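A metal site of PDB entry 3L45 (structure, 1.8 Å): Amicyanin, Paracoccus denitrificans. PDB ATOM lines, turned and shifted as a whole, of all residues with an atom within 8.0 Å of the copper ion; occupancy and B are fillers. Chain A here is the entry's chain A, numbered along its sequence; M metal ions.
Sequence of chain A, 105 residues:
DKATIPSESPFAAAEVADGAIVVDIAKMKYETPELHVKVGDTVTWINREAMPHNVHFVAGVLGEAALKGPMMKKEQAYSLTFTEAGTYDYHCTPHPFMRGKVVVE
Of the 22 residues printed, 4 come within 4 Å of the copper ion.
The nearest printed residue that does not touch the copper ion is Pro 52 (4.1 Å).
The copper ion is bound by a ring nitrogen (ND1) of His 53 (2.0 Å), the side-chain sulfur of Cys 92 (2.1 Å) and a ring nitrogen (ND1) of His 95 (2.4 Å).
Slightly farther from the copper ion lies SD of Met 98 (2.8 Å).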
ATOM      1  N   ILE A  25     -27.448  -4.187 -27.706  1.00  0.00           N
ATOM      2  CA  ILE A  25     -27.290  -4.869 -26.424  1.00  0.00           C
ATOM      3  C   ILE A  25     -28.626  -5.541 -26.183  1.00  0.00           C
ATOM      4  O   ILE A  25     -29.674  -4.886 -26.195  1.00  0.00           O
ATOM      5  CB  ILE A  25     -26.952  -3.892 -25.316  1.00  0.00           C
ATOM      6  CG1 ILE A  25     -25.700  -3.096 -25.648  1.00  0.00           C
ATOM      7  CG2 ILE A  25     -26.754  -4.627 -24.017  1.00  0.00           C
ATOM      8  CD1 ILE A  25     -25.290  -2.124 -24.552  1.00  0.00           C
ATOM      9  N   MET A  28     -28.746  -9.716 -22.301  1.00  0.00           N
ATOM     10  CA  MET A  28     -27.576  -9.623 -21.420  1.00  0.00           C
ATOM     11  C   MET A  28     -26.260  -9.873 -22.140  1.00  0.00           C
ATOM     12  O   MET A  28     -25.314 -10.394 -21.554  1.00  0.00           O
ATOM     13  CB  MET A  28     -27.697 -10.584 -20.233  1.00  0.00           C
ATOM     14  CG  MET A  28     -28.870 -10.337 -19.280  1.00  0.00           C
ATOM     15  SD  MET A  28     -29.189  -8.702 -18.561  1.00  0.00           S
ATOM     16  CE  MET A  28     -28.199  -8.742 -17.032  1.00  0.00           C
ATOM     17  N   LYS A  29     -26.193  -9.450 -23.391  1.00  0.00           N
ATOM     18  CA  LYS A  29     -24.959  -9.575 -24.152  1.00  0.00           C
ATOM     19  C   LYS A  29     -24.758  -8.366 -25.083  1.00  0.00           C
ATOM     20  O   LYS A  29     -25.732  -7.875 -25.652  1.00  0.00           O
ATOM     21  CB  LYS A  29     -24.980 -10.854 -25.024  1.00  0.00           C
ATOM     22  CG  LYS A  29     -25.170 -12.198 -24.317  1.00  0.00           C
ATOM     23  CD  LYS A  29     -25.044 -13.364 -25.312  1.00  0.00           C
ATOM     24  CE  LYS A  29     -25.172 -14.742 -24.635  1.00  0.00           C
ATOM     25  NZ  LYS A  29     -26.616 -15.034 -24.386  1.00  0.00           N
ATOM     26  N   TYR A  30     -23.489  -8.039 -25.392  1.00  0.00           N
ATOM     27  CA  TYR A  30     -23.212  -7.079 -26.453  1.00  0.00           C
ATOM     28  C   TYR A  30     -23.273  -7.996 -27.730  1.00  0.00           C
ATOM     29  O   TYR A  30     -22.583  -9.045 -27.799  1.00  0.00           O
ATOM     30  CB  TYR A  30     -21.835  -6.469 -26.301  1.00  0.00           C
ATOM     31  CG  TYR A  30     -21.668  -5.644 -25.049  1.00  0.00           C
ATOM     32  CD1 TYR A  30     -22.299  -4.427 -24.884  1.00  0.00           C
ATOM     33  CD2 TYR A  30     -20.833  -6.097 -23.989  1.00  0.00           C
ATOM     34  CE1 TYR A  30     -22.106  -3.692 -23.701  1.00  0.00           C
ATOM     35  CE2 TYR A  30     -20.650  -5.369 -22.847  1.00  0.00           C
ATOM     36  CZ  TYR A  30     -21.272  -4.193 -22.704  1.00  0.00           C
ATOM     37  OH  TYR A  30     -21.054  -3.467 -21.580  1.00  0.00           O
ATOM     38  N   ASN A  47     -29.197   0.059 -26.243  1.00  0.00           N
ATOM     39  CA  ASN A  47     -29.780  -0.902 -25.338  1.00  0.00           C
ATOM     40  C   ASN A  47     -31.158  -1.242 -25.895  1.00  0.00           C
ATOM     41  O   ASN A  47     -31.979  -0.354 -26.060  1.00  0.00           O
ATOM     42  CB  ASN A  47     -29.880  -0.362 -23.936  1.00  0.00           C
ATOM     43  CG  ASN A  47     -30.284  -1.449 -22.954  1.00  0.00           C
ATOM     44  OD1 ASN A  47     -30.382  -2.635 -23.332  1.00  0.00           O
ATOM     45  ND2 ASN A  47     -30.595  -1.064 -21.745  1.00  0.00           N
ATOM     46  N   GLU A  49     -33.145  -3.629 -24.487  1.00  0.00           N
ATOM     47  CA  GLU A  49     -33.900  -4.338 -23.463  1.00  0.00           C
ATOM     48  C   GLU A  49     -34.141  -3.487 -22.262  1.00  0.00           C
ATOM     49  O   GLU A  49     -33.440  -2.501 -22.089  1.00  0.00           O
ATOM     50  CB  GLU A  49     -33.262  -5.701 -23.137  1.00  0.00           C
ATOM     51  CG  GLU A  49     -31.981  -5.691 -22.339  1.00  0.00           C
ATOM     52  CD  GLU A  49     -31.411  -7.113 -22.158  1.00  0.00           C
ATOM     53  OE1 GLU A  49     -32.172  -8.090 -22.340  1.00  0.00           O
ATOM     54  OE2 GLU A  49     -30.218  -7.270 -21.837  1.00  0.00           O
ATOM     55  N   MET A  51     -33.618  -3.952 -19.076  1.00  0.00           N
ATOM     56  CA  MET A  51     -32.583  -3.911 -18.058  1.00  0.00           C
ATOM     57  C   MET A  51     -31.527  -2.893 -18.468  1.00  0.00           C
ATOM     58  O   MET A  51     -30.984  -3.010 -19.564  1.00  0.00           O
ATOM     59  CB  MET A  51     -31.931  -5.302 -17.963  1.00  0.00           C
ATOM     60  CG  MET A  51     -30.718  -5.384 -17.044  1.00  0.00           C
ATOM     61  SD  MET A  51     -31.171  -4.964 -15.328  1.00  0.00           S
ATOM     62  CE  MET A  51     -31.412  -6.558 -14.495  1.00  0.00           C
ATOM     63  N   PRO A  52     -31.229  -1.885 -17.614  1.00  0.00           N
ATOM     64  CA  PRO A  52     -30.186  -0.933 -18.021  1.00  0.00           C
ATOM     65  C   PRO A  52     -28.786  -1.525 -18.120  1.00  0.00           C
ATOM     66  O   PRO A  52     -28.413  -2.430 -17.379  1.00  0.00           O
ATOM     67  CB  PRO A  52     -30.204   0.134 -16.936  1.00  0.00           C
ATOM     68  CG  PRO A  52     -31.464  -0.080 -16.143  1.00  0.00           C
ATOM     69  CD  PRO A  52     -31.819  -1.535 -16.310  1.00  0.00           C
ATOM     70  N   HIS A  53     -28.017  -0.994 -19.051  1.00  0.00           N
ATOM     71  CA  HIS A  53     -26.644  -1.438 -19.308  1.00  0.00           C
ATOM     72  C   HIS A  53     -25.792  -0.257 -19.674  1.00  0.00           C
ATOM     73  O   HIS A  53     -26.297   0.772 -20.118  1.00  0.00           O
ATOM     74  CB  HIS A  53     -26.576  -2.371 -20.486  1.00  0.00           C
ATOM     75  CG  HIS A  53     -27.399  -3.615 -20.340  1.00  0.00           C
ATOM     76  ND1 HIS A  53     -27.009  -4.662 -19.551  1.00  0.00           N
ATOM     77  CD2 HIS A  53     -28.485  -4.036 -21.042  1.00  0.00           C
ATOM     78  CE1 HIS A  53     -27.802  -5.689 -19.765  1.00  0.00           C
ATOM     79  NE2 HIS A  53     -28.701  -5.348 -20.673  1.00  0.00           N
ATOM     80  N   ASN A  54     -24.467  -0.424 -19.532  1.00  0.00           N
ATOM     81  CA  ASN A  54     -23.508   0.646 -19.940  1.00  0.00           C
ATOM     82  C   ASN A  54     -22.287   0.006 -20.513  1.00  0.00           C
ATOM     83  O   ASN A  54     -22.222  -1.210 -20.680  1.00  0.00           O
ATOM     84  CB  ASN A  54     -23.130   1.611 -18.797  1.00  0.00           C
ATOM     85  CG  ASN A  54     -22.165   1.002 -17.793  1.00  0.00           C
ATOM     86  OD1 ASN A  54     -21.996  -0.218 -17.717  1.00  0.00           O
ATOM     87  ND2 ASN A  54     -21.524   1.853 -17.024  1.00  0.00           N
ATOM     88  N   VAL A  55     -21.280   0.828 -20.798  1.00  0.00           N
ATOM     89  CA  VAL A  55     -19.978   0.359 -21.277  1.00  0.00           C
ATOM     90  C   VAL A  55     -19.040   1.036 -20.324  1.00  0.00           C
ATOM     91  O   VAL A  55     -19.247   2.200 -19.967  1.00  0.00           O
ATOM     92  CB  VAL A  55     -19.619   0.676 -22.736  1.00  0.00           C
ATOM     93  CG1 VAL A  55     -20.481  -0.192 -23.649  1.00  0.00           C
ATOM     94  CG2 VAL A  55     -19.820   2.128 -23.034  1.00  0.00           C
ATOM     95  N   MET A  71     -25.740   4.925 -17.583  1.00  0.00           N
ATOM     96  CA  MET A  71     -26.635   3.796 -17.765  1.00  0.00           C
ATOM     97  C   MET A  71     -27.626   4.117 -18.849  1.00  0.00           C
ATOM     98  O   MET A  71     -28.237   5.193 -18.849  1.00  0.00           O
ATOM     99  CB  MET A  71     -27.352   3.415 -16.490  1.00  0.00           C
ATOM    100  CG  MET A  71     -26.419   3.022 -15.377  1.00  0.00           C
ATOM    101  SD  MET A  71     -25.266   1.673 -15.736  1.00  0.00           S
ATOM    102  CE  MET A  71     -26.307   0.391 -15.813  1.00  0.00           C
ATOM    103  N   MET A  72     -27.800   3.196 -19.776  1.00  0.00           N
ATOM    104  CA  MET A  72     -28.764   3.381 -20.881  1.00  0.00           C
ATOM    105  C   MET A  72     -30.053   2.636 -20.517  1.00  0.00           C
ATOM    106  O   MET A  72     -30.010   1.445 -20.163  1.00  0.00           O
ATOM    107  CB  MET A  72     -28.187   2.790 -22.183  1.00  0.00           C
ATOM    108  CG  MET A  72     -26.992   3.492 -22.724  1.00  0.00           C
ATOM    109  SD  MET A  72     -26.357   2.668 -24.191  1.00  0.00           S
ATOM    110  CE  MET A  72     -25.416   1.482 -23.385  1.00  0.00           C
ATOM    111  N   HIS A  91     -16.593  -3.557 -20.394  1.00  0.00           N
ATOM    112  CA  HIS A  91     -17.546  -4.436 -19.737  1.00  0.00           C
ATOM    113  C   HIS A  91     -18.699  -3.584 -19.231  1.00  0.00           C
ATOM    114  O   HIS A  91     -18.673  -2.356 -19.281  1.00  0.00           O
ATOM    115  CB  HIS A  91     -16.903  -5.214 -18.573  1.00  0.00           C
ATOM    116  CG  HIS A  91     -16.584  -4.367 -17.377  1.00  0.00           C
ATOM    117  ND1 HIS A  91     -15.446  -3.581 -17.295  1.00  0.00           N
ATOM    118  CD2 HIS A  91     -17.246  -4.175 -16.216  1.00  0.00           C
ATOM    119  CE1 HIS A  91     -15.440  -2.940 -16.137  1.00  0.00           C
ATOM    120  NE2 HIS A  91     -16.528  -3.280 -15.474  1.00  0.00           N
ATOM    121  N   CYS A  92     -19.710  -4.253 -18.732  1.00  0.00           N
ATOM    122  CA  CYS A  92     -20.900  -3.588 -18.189  1.00  0.00           C
ATOM    123  C   CYS A  92     -20.728  -3.460 -16.669  1.00  0.00           C
ATOM    124  O   CYS A  92     -20.486  -4.457 -15.997  1.00  0.00           O
ATOM    125  CB  CYS A  92     -22.157  -4.363 -18.547  1.00  0.00           C
ATOM    126  SG  CYS A  92     -23.602  -3.620 -17.853  1.00  0.00           S
ATOM    127  N   THR A  93     -20.793  -2.243 -16.130  1.00  0.00           N
ATOM    128  CA  THR A  93     -20.569  -2.023 -14.696  1.00  0.00           C
ATOM    129  C   THR A  93     -21.408  -2.934 -13.813  1.00  0.00           C
ATOM    130  O   THR A  93     -20.849  -3.745 -13.071  1.00  0.00           O
ATOM    131  CB  THR A  93     -20.723  -0.559 -14.293  1.00  0.00           C
ATOM    132  OG1 THR A  93     -19.926   0.281 -15.119  1.00  0.00           O
ATOM    133  CG2 THR A  93     -20.249  -0.305 -12.815  1.00  0.00           C
ATOM    134  N   PRO A  94     -22.740  -2.862 -13.891  1.00  0.00           N
ATOM    135  CA  PRO A  94     -23.505  -3.795 -13.037  1.00  0.00           C
ATOM    136  C   PRO A  94     -23.447  -5.294 -13.383  1.00  0.00           C
ATOM    137  O   PRO A  94     -23.805  -6.144 -12.556  1.00  0.00           O
ATOM    138  CB  PRO A  94     -24.931  -3.295 -13.151  1.00  0.00           C
ATOM    139  CG  PRO A  94     -24.992  -2.699 -14.518  1.00  0.00           C
ATOM    140  CD  PRO A  94     -23.657  -1.985 -14.657  1.00  0.00           C
ATOM    141  N   HIS A  95     -23.036  -5.623 -14.599  1.00  0.00           N
ATOM    142  CA  HIS A  95     -22.990  -7.011 -15.068  1.00  0.00           C
ATOM    143  C   HIS A  95     -21.625  -7.265 -15.713  1.00  0.00           C
ATOM    144  O   HIS A  95     -21.533  -7.397 -16.916  1.00  0.00           O
ATOM    145  CB  HIS A  95     -24.073  -7.222 -16.137  1.00  0.00           C
ATOM    146  CG  HIS A  95     -25.412  -6.689 -15.781  1.00  0.00           C
ATOM    147  ND1 HIS A  95     -26.119  -5.860 -16.637  1.00  0.00           N
ATOM    148  CD2 HIS A  95     -26.227  -6.848 -14.699  1.00  0.00           C
ATOM    149  CE1 HIS A  95     -27.273  -5.538 -16.117  1.00  0.00           C
ATOM    150  NE2 HIS A  95     -27.376  -6.127 -14.937  1.00  0.00           N
ATOM    151  N   PRO A  96     -20.543  -7.330 -14.918  1.00  0.00           N
ATOM    152  CA  PRO A  96     -19.181  -7.516 -15.446  1.00  0.00           C
ATOM    153  C   PRO A  96     -18.936  -8.766 -16.265  1.00  0.00           C
ATOM    154  O   PRO A  96     -17.929  -8.867 -16.988  1.00  0.00           O
ATOM    155  CB  PRO A  96     -18.313  -7.463 -14.206  1.00  0.00           C
ATOM    156  CG  PRO A  96     -19.219  -7.885 -13.118  1.00  0.00           C
ATOM    157  CD  PRO A  96     -20.522  -7.204 -13.451  1.00  0.00           C
ATOM    158  N   PHE A  97     -19.884  -9.703 -16.203  1.00  0.00           N
ATOM    159  CA  PHE A  97     -19.762 -10.894 -17.071  1.00  0.00           C
ATOM    160  C   PHE A  97     -19.976 -10.522 -18.555  1.00  0.00           C
ATOM    161  O   PHE A  97     -19.586 -11.292 -19.455  1.00  0.00           O
ATOM    162  CB  PHE A  97     -20.713 -12.011 -16.621  1.00  0.00           C
ATOM    163  CG  PHE A  97     -22.149 -11.591 -16.504  1.00  0.00           C
ATOM    164  CD1 PHE A  97     -22.974 -11.474 -17.614  1.00  0.00           C
ATOM    165  CD2 PHE A  97     -22.671 -11.299 -15.258  1.00  0.00           C
ATOM    166  CE1 PHE A  97     -24.274 -11.079 -17.473  1.00  0.00           C
ATOM    167  CE2 PHE A  97     -23.937 -10.920 -15.090  1.00  0.00           C
ATOM    168  CZ  PHE A  97     -24.767 -10.798 -16.212  1.00  0.00           C
ATOM    169  N   MET A  98     -20.555  -9.331 -18.791  1.00  0.00           N
ATOM    170  CA  MET A  98     -20.798  -8.793 -20.154  1.00  0.00           C
ATOM    171  C   MET A  98     -19.571  -8.070 -20.548  1.00  0.00           C
ATOM    172  O   MET A  98     -19.165  -7.128 -19.894  1.00  0.00           O
ATOM    173  CB  MET A  98     -21.939  -7.790 -20.213  1.00  0.00           C
ATOM    174  CG  MET A  98     -23.233  -8.380 -19.898  1.00  0.00           C
ATOM    175  SD  MET A  98     -24.536  -7.152 -19.881  1.00  0.00           S
ATOM    176  CE  MET A  98     -24.721  -6.746 -21.533  1.00  0.00           C
ATOM    177  N   ARG A  99     -18.938  -8.595 -21.553  1.00  0.00           N
ATOM    178  CA  ARG A  99     -17.646  -8.109 -21.989  1.00  0.00           C
ATOM    179  C   ARG A  99     -17.608  -7.983 -23.501  1.00  0.00           C
ATOM    180  O   ARG A  99     -18.233  -8.751 -24.208  1.00  0.00           O
ATOM    181  CB  ARG A  99     -16.522  -9.088 -21.573  1.00  0.00           C
ATOM    182  CG  ARG A  99     -16.491  -9.303 -20.091  1.00  0.00           C
ATOM    183  CD  ARG A  99     -15.182  -8.968 -19.494  1.00  0.00           C
ATOM    184  NE  ARG A  99     -15.388  -8.685 -18.068  1.00  0.00           N
ATOM    185  CZ  ARG A  99     -14.523  -8.030 -17.300  1.00  0.00           C
ATOM    186  NH1 ARG A  99     -13.287  -7.706 -17.738  1.00  0.00           N
ATOM    187  NH2 ARG A  99     -14.920  -7.706 -16.076  1.00  0.00           N
HETATM  188 CU    CU M   1     -25.244  -4.754 -18.544  1.00  0.00          CU
